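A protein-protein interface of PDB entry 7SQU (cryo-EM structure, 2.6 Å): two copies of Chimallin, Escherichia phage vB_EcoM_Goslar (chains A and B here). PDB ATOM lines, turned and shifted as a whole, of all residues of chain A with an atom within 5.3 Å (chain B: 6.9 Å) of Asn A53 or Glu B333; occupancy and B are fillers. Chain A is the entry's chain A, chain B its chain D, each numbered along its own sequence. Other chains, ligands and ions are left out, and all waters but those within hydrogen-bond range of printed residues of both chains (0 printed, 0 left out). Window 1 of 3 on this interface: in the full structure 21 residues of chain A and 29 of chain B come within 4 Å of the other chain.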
ATOM      1  N   ARG A  50      16.779  -0.640 -15.688  1.00  0.00           N
ATOM      2  CA  ARG A  50      17.688  -1.611 -15.087  1.00  0.00           C
ATOM      3  C   ARG A  50      17.294  -3.040 -15.433  1.00  0.00           C
ATOM      4  O   ARG A  50      18.163  -3.908 -15.584  1.00  0.00           O
ATOM      5  CB  ARG A  50      17.746  -1.423 -13.574  1.00  0.00           C
ATOM      6  CG  ARG A  50      18.808  -0.450 -13.110  1.00  0.00           C
ATOM      7  CD  ARG A  50      18.445   0.991 -13.406  1.00  0.00           C
ATOM      8  NE  ARG A  50      17.334   1.456 -12.585  1.00  0.00           N
ATOM      9  CZ  ARG A  50      17.435   1.773 -11.303  1.00  0.00           C
ATOM     10  NH1 ARG A  50      18.583   1.685 -10.654  1.00  0.00           N
ATOM     11  NH2 ARG A  50      16.351   2.192 -10.655  1.00  0.00           N
ATOM     12  N   THR A  51      16.001  -3.317 -15.550  1.00  0.00           N
ATOM     13  CA  THR A  51      15.507  -4.661 -15.811  1.00  0.00           C
ATOM     14  C   THR A  51      14.979  -4.813 -17.233  1.00  0.00           C
ATOM     15  O   THR A  51      14.082  -5.615 -17.484  1.00  0.00           O
ATOM     16  CB  THR A  51      14.421  -5.032 -14.807  1.00  0.00           C
ATOM     17  OG1 THR A  51      13.370  -4.061 -14.865  1.00  0.00           O
ATOM     18  CG2 THR A  51      14.993  -5.074 -13.403  1.00  0.00           C
ATOM     19  N   ILE A  52      15.544  -4.056 -18.172  1.00  0.00           N
ATOM     20  CA  ILE A  52      15.085  -4.092 -19.558  1.00  0.00           C
ATOM     21  C   ILE A  52      15.288  -5.475 -20.173  1.00  0.00           C
ATOM     22  O   ILE A  52      14.455  -5.945 -20.955  1.00  0.00           O
ATOM     23  CB  ILE A  52      15.764  -2.980 -20.377  1.00  0.00           C
ATOM     24  CG1 ILE A  52      15.110  -2.858 -21.747  1.00  0.00           C
ATOM     25  CG2 ILE A  52      17.259  -3.200 -20.495  1.00  0.00           C
ATOM     26  CD1 ILE A  52      13.707  -2.359 -21.688  1.00  0.00           C
ATOM     27  N   ASN A  53      16.393  -6.139 -19.848  1.00  0.00           N
ATOM     28  CA  ASN A  53      16.662  -7.457 -20.417  1.00  0.00           C
ATOM     29  C   ASN A  53      15.620  -8.484 -19.989  1.00  0.00           C
ATOM     30  O   ASN A  53      15.258  -9.363 -20.772  1.00  0.00           O
ATOM     31  CB  ASN A  53      18.075  -7.907 -20.076  1.00  0.00           C
ATOM     32  CG  ASN A  53      19.118  -7.190 -20.902  1.00  0.00           C
ATOM     33  OD1 ASN A  53      18.795  -6.511 -21.867  1.00  0.00           O
ATOM     34  ND2 ASN A  53      20.374  -7.333 -20.527  1.00  0.00           N
ATOM     35  N   ARG A  54      15.165  -8.429 -18.736  1.00  0.00           N
ATOM     36  CA  ARG A  54      14.098  -9.328 -18.306  1.00  0.00           C
ATOM     37  C   ARG A  54      12.787  -9.045 -19.031  1.00  0.00           C
ATOM     38  O   ARG A  54      12.049  -9.977 -19.362  1.00  0.00           O
ATOM     39  CB  ARG A  54      13.905  -9.260 -16.798  1.00  0.00           C
ATOM     40  CG  ARG A  54      15.122  -9.689 -16.035  1.00  0.00           C
ATOM     41  CD  ARG A  54      14.910  -9.627 -14.538  1.00  0.00           C
ATOM     42  NE  ARG A  54      14.184  -8.440 -14.096  1.00  0.00           N
ATOM     43  CZ  ARG A  54      12.909  -8.438 -13.727  1.00  0.00           C
ATOM     44  NH1 ARG A  54      12.187  -9.545 -13.734  1.00  0.00           N
ATOM     45  NH2 ARG A  54      12.350  -7.298 -13.335  1.00  0.00           N
ATOM     46  N   THR A  55      12.457  -7.776 -19.260  1.00  0.00           N
ATOM     47  CA  THR A  55      11.249  -7.469 -20.016  1.00  0.00           C
ATOM     48  C   THR A  55      11.381  -7.937 -21.462  1.00  0.00           C
ATOM     49  O   THR A  55      10.631  -8.806 -21.914  1.00  0.00           O
ATOM     50  CB  THR A  55      10.959  -5.969 -19.957  1.00  0.00           C
ATOM     51  OG1 THR A  55      11.002  -5.527 -18.600  1.00  0.00           O
ATOM     52  CG2 THR A  55       9.598  -5.660 -20.530  1.00  0.00           C
ATOM     53  N   LEU A  56      12.303  -7.347 -22.215  1.00  0.00           N
ATOM     54  CA  LEU A  56      12.536  -7.728 -23.607  1.00  0.00           C
ATOM     55  C   LEU A  56      13.683  -8.734 -23.633  1.00  0.00           C
ATOM     56  O   LEU A  56      14.842  -8.369 -23.800  1.00  0.00           O
ATOM     57  CB  LEU A  56      12.845  -6.498 -24.449  1.00  0.00           C
ATOM     58  CG  LEU A  56      12.018  -5.247 -24.163  1.00  0.00           C
ATOM     59  CD1 LEU A  56      12.525  -4.071 -24.962  1.00  0.00           C
ATOM     60  CD2 LEU A  56      10.568  -5.494 -24.488  1.00  0.00           C
ATOM     61  N   SER A  57      13.366 -10.014 -23.477  1.00  0.00           N
ATOM     62  CA  SER A  57      14.392 -11.036 -23.308  1.00  0.00           C
ATOM     63  C   SER A  57      14.671 -11.803 -24.594  1.00  0.00           C
ATOM     64  O   SER A  57      13.854 -11.853 -25.512  1.00  0.00           O
ATOM     65  CB  SER A  57      13.991 -12.014 -22.206  1.00  0.00           C
ATOM     66  OG  SER A  57      12.747 -12.615 -22.486  1.00  0.00           O
ATOM     67  N   ARG A  58      15.856 -12.419 -24.634  1.00  0.00           N
ATOM     68  CA  ARG A  58      16.282 -13.288 -25.719  1.00  0.00           C
ATOM     69  C   ARG A  58      16.913 -14.543 -25.132  1.00  0.00           C
ATOM     70  O   ARG A  58      17.451 -14.523 -24.026  1.00  0.00           O
ATOM     71  CB  ARG A  58      17.271 -12.569 -26.639  1.00  0.00           C
ATOM     72  CG  ARG A  58      16.675 -11.396 -27.388  1.00  0.00           C
ATOM     73  CD  ARG A  58      15.682 -11.852 -28.416  1.00  0.00           C
ATOM     74  NE  ARG A  58      15.179 -10.767 -29.245  1.00  0.00           N
ATOM     75  CZ  ARG A  58      13.994 -10.204 -29.084  1.00  0.00           C
ATOM     76  NH1 ARG A  58      13.183 -10.575 -28.114  1.00  0.00           N
ATOM     77  NH2 ARG A  58      13.603  -9.261 -29.931  1.00  0.00           N
ATOM     78  N   ASN A  63      26.747 -11.441 -24.156  1.00  0.00           N
ATOM     79  CA  ASN A  63      27.504 -10.997 -22.954  1.00  0.00           C
ATOM     80  C   ASN A  63      27.084 -11.846 -21.745  1.00  0.00           C
ATOM     81  O   ASN A  63      25.890 -11.822 -21.393  1.00  0.00           O
ATOM     82  CB  ASN A  63      27.351  -9.492 -22.716  1.00  0.00           C
ATOM     83  CG  ASN A  63      26.001  -8.935 -23.122  1.00  0.00           C
ATOM     84  OD1 ASN A  63      24.997  -9.645 -23.129  1.00  0.00           O
ATOM     85  ND2 ASN A  63      25.962  -7.655 -23.450  1.00  0.00           N
ATOM     86  N   ALA A 132      31.761  -0.583 -17.181  1.00  0.00           N
ATOM     87  CA  ALA A 132      31.758   0.697 -17.870  1.00  0.00           C
ATOM     88  C   ALA A 132      32.410   1.770 -17.001  1.00  0.00           C
ATOM     89  O   ALA A 132      32.258   1.754 -15.781  1.00  0.00           O
ATOM     90  CB  ALA A 132      30.336   1.116 -18.215  1.00  0.00           C
ATOM     91  N   GLN B 281      26.764   4.103 -15.057  1.00  0.00           N
ATOM     92  CA  GLN B 281      26.085   4.333 -16.316  1.00  0.00           C
ATOM     93  C   GLN B 281      25.844   2.999 -16.996  1.00  0.00           C
ATOM     94  O   GLN B 281      26.521   2.010 -16.727  1.00  0.00           O
ATOM     95  CB  GLN B 281      26.873   5.266 -17.226  1.00  0.00           C
ATOM     96  CG  GLN B 281      27.960   4.597 -18.003  1.00  0.00           C
ATOM     97  CD  GLN B 281      28.753   5.572 -18.822  1.00  0.00           C
ATOM     98  OE1 GLN B 281      28.201   6.465 -19.439  1.00  0.00           O
ATOM     99  NE2 GLN B 281      30.062   5.419 -18.816  1.00  0.00           N
ATOM    100  N   GLN B 282      24.848   2.980 -17.874  1.00  0.00           N
ATOM    101  CA  GLN B 282      24.435   1.786 -18.597  1.00  0.00           C
ATOM    102  C   GLN B 282      24.383   2.127 -20.075  1.00  0.00           C
ATOM    103  O   GLN B 282      23.622   3.007 -20.479  1.00  0.00           O
ATOM    104  CB  GLN B 282      23.075   1.322 -18.091  1.00  0.00           C
ATOM    105  CG  GLN B 282      22.437   0.210 -18.854  1.00  0.00           C
ATOM    106  CD  GLN B 282      21.011   0.000 -18.420  1.00  0.00           C
ATOM    107  OE1 GLN B 282      20.334   0.939 -18.027  1.00  0.00           O
ATOM    108  NE2 GLN B 282      20.547  -1.233 -18.485  1.00  0.00           N
ATOM    109  N   ARG B 283      25.176   1.430 -20.882  1.00  0.00           N
ATOM    110  CA  ARG B 283      25.332   1.770 -22.290  1.00  0.00           C
ATOM    111  C   ARG B 283      24.364   0.976 -23.150  1.00  0.00           C
ATOM    112  O   ARG B 283      24.297  -0.249 -23.050  1.00  0.00           O
ATOM    113  CB  ARG B 283      26.766   1.514 -22.735  1.00  0.00           C
ATOM    114  CG  ARG B 283      27.785   2.173 -21.846  1.00  0.00           C
ATOM    115  CD  ARG B 283      29.082   2.354 -22.564  1.00  0.00           C
ATOM    116  NE  ARG B 283      29.951   1.204 -22.384  1.00  0.00           N
ATOM    117  CZ  ARG B 283      31.266   1.278 -22.233  1.00  0.00           C
ATOM    118  NH1 ARG B 283      31.896   2.440 -22.247  1.00  0.00           N
ATOM    119  NH2 ARG B 283      31.965   0.160 -22.064  1.00  0.00           N
ATOM    120  N   LEU B 284      23.634   1.675 -24.016  1.00  0.00           N
ATOM    121  CA  LEU B 284      22.545   1.068 -24.770  1.00  0.00           C
ATOM    122  C   LEU B 284      22.898   0.761 -26.223  1.00  0.00           C
ATOM    123  O   LEU B 284      22.856  -0.400 -26.626  1.00  0.00           O
ATOM    124  CB  LEU B 284      21.314   1.970 -24.687  1.00  0.00           C
ATOM    125  CG  LEU B 284      20.930   2.319 -23.253  1.00  0.00           C
ATOM    126  CD1 LEU B 284      19.877   3.377 -23.223  1.00  0.00           C
ATOM    127  CD2 LEU B 284      20.465   1.100 -22.510  1.00  0.00           C
ATOM    128  N   VAL B 285      23.269   1.766 -27.015  1.00  0.00           N
ATOM    129  CA  VAL B 285      23.382   1.596 -28.461  1.00  0.00           C
ATOM    130  C   VAL B 285      24.502   2.478 -29.000  1.00  0.00           C
ATOM    131  O   VAL B 285      24.857   3.492 -28.406  1.00  0.00           O
ATOM    132  CB  VAL B 285      22.021   1.904 -29.131  1.00  0.00           C
ATOM    133  CG1 VAL B 285      21.684   3.353 -28.999  1.00  0.00           C
ATOM    134  CG2 VAL B 285      22.021   1.503 -30.574  1.00  0.00           C
ATOM    135  N   PRO B 331      23.560  -2.861 -30.821  1.00  0.00           N
ATOM    136  CA  PRO B 331      23.382  -2.718 -29.374  1.00  0.00           C
ATOM    137  C   PRO B 331      24.657  -2.976 -28.587  1.00  0.00           C
ATOM    138  O   PRO B 331      25.602  -3.601 -29.063  1.00  0.00           O
ATOM    139  CB  PRO B 331      22.336  -3.782 -29.052  1.00  0.00           C
ATOM    140  CG  PRO B 331      22.547  -4.810 -30.071  1.00  0.00           C
ATOM    141  CD  PRO B 331      22.970  -4.112 -31.319  1.00  0.00           C
ATOM    142  N   LEU B 332      24.665  -2.477 -27.352  1.00  0.00           N
ATOM    143  CA  LEU B 332      25.814  -2.615 -26.466  1.00  0.00           C
ATOM    144  C   LEU B 332      25.528  -3.511 -25.269  1.00  0.00           C
ATOM    145  O   LEU B 332      26.172  -4.546 -25.107  1.00  0.00           O
ATOM    146  CB  LEU B 332      26.281  -1.238 -25.994  1.00  0.00           C
ATOM    147  CG  LEU B 332      26.985  -0.386 -27.041  1.00  0.00           C
ATOM    148  CD1 LEU B 332      27.113   1.033 -26.561  1.00  0.00           C
ATOM    149  CD2 LEU B 332      28.336  -0.960 -27.357  1.00  0.00           C
ATOM    150  N   GLU B 333      24.566  -3.149 -24.431  1.00  0.00           N
ATOM    151  CA  GLU B 333      24.166  -3.985 -23.312  1.00  0.00           C
ATOM    152  C   GLU B 333      22.716  -4.422 -23.412  1.00  0.00           C
ATOM    153  O   GLU B 333      22.247  -5.149 -22.535  1.00  0.00           O
ATOM    154  CB  GLU B 333      24.391  -3.265 -21.980  1.00  0.00           C
ATOM    155  CG  GLU B 333      25.849  -3.074 -21.630  1.00  0.00           C
ATOM    156  CD  GLU B 333      26.046  -2.353 -20.317  1.00  0.00           C
ATOM    157  OE1 GLU B 333      25.185  -2.491 -19.428  1.00  0.00           O
ATOM    158  OE2 GLU B 333      27.055  -1.636 -20.176  1.00  0.00           O
ATOM    159  N   LEU B 334      21.998  -3.985 -24.435  1.00  0.00           N
ATOM    160  CA  LEU B 334      20.650  -4.462 -24.679  1.00  0.00           C
ATOM    161  C   LEU B 334      20.705  -5.827 -25.337  1.00  0.00           C
ATOM    162  O   LEU B 334      21.538  -6.074 -26.209  1.00  0.00           O
ATOM    163  CB  LEU B 334      19.890  -3.497 -25.580  1.00  0.00           C
ATOM    164  CG  LEU B 334      19.530  -2.143 -25.001  1.00  0.00           C
ATOM    165  CD1 LEU B 334      18.840  -1.310 -26.041  1.00  0.00           C
ATOM    166  CD2 LEU B 334      18.634  -2.342 -23.815  1.00  0.00           C
ATOM    167  N   ASP B 335      19.837  -6.728 -24.894  1.00  0.00           N
ATOM    168  CA  ASP B 335      19.778  -8.044 -25.512  1.00  0.00           C
ATOM    169  C   ASP B 335      19.032  -8.029 -26.837  1.00  0.00           C
ATOM    170  O   ASP B 335      19.393  -8.776 -27.748  1.00  0.00           O
ATOM    171  CB  ASP B 335      19.127  -9.040 -24.560  1.00  0.00           C
ATOM    172  CG  ASP B 335      20.113  -9.628 -23.582  1.00  0.00           C
ATOM    173  OD1 ASP B 335      21.329  -9.434 -23.772  1.00  0.00           O
ATOM    174  OD2 ASP B 335      19.675 -10.287 -22.618  1.00  0.00           O
ATOM    175  N   ALA B 336      18.017  -7.187 -26.979  1.00  0.00           N
ATOM    176  CA  ALA B 336      17.168  -7.171 -28.156  1.00  0.00           C
ATOM    177  C   ALA B 336      17.391  -5.902 -28.963  1.00  0.00           C
ATOM    178  O   ALA B 336      17.577  -4.824 -28.399  1.00  0.00           O
ATOM    179  CB  ALA B 336      15.696  -7.269 -27.762  1.00  0.00           C
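The side-chain amide oxygen (OD1) of Asn A53 is in hydrogen-bond range of the backbone NH (N) of Asp B335.
The backbone NH (N) of Leu B332 is in hydrogen-bond range of the backbone carbonyl oxygen (O) of Leu B284, at 2.8 Å. The backbone carbonyl oxygen (O) of Arg B283 sits close to the backbone NH (N) of Glu B333, at 3.2 Å.
Among the printed residues, pairs that only touch across the chains: Ile A52 with Leu B334 (3.7 Å), Asn A53 with Glu B333 (3.5 Å), Asn A53 with Leu B334 (3.9 Å), Arg A58 with Asp B335 (3.8 Å), Arg A58 with Ala B336 (3.6 Å), Asn A63 with Leu B332 (3.5 Å) and Asn A63 with Asp B335 (3.7 Å).
Asn A53 touches just these residues of chain B: Glu B333 (3.5 Å), Leu B334 (3.9 Å) and Asp B335 (3.2 Å). Leu A56 touches none of the printed residues of chain B. Printed residues of chain B within 4 Å of Asn A63: Leu B332 (3.5 Å) and Asp B335 (3.7 Å). Of chain A, only Asn A53 comes within 4 Å of Glu B333. Of the printed residues of chain A, Leu B334 touches Ile A52 (3.7 Å) and Asn A53 (3.9 Å). Printed residues of chain A within 4 Å of Ala B336: Arg A58. The nearest residue of chain B that does not touch Asn A53 is Ala B336 (5.2 Å). The nearest printed residue of chain A that does not touch Ala B336 is Leu A56 (4.2 Å).
Hydrophobic or aromatic side chains of chain A within 4 Å of the printed part of chain B: Ile A52. Of the 11 printed residues of chain B, 5 touch a printed residue of chain A. Printed residues of chain B that touch a printed residue of chain A: Leu B332, Glu B333, Leu B334, Asp B335 and Ala B336. Among the printed residues, 8 pairs touch across the chains. Among the printed residues, no Asp or Glu carboxylate lies within 4 Å of a Lys or Arg side-chain nitrogen of the other chain.
No position is printed for both chains.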
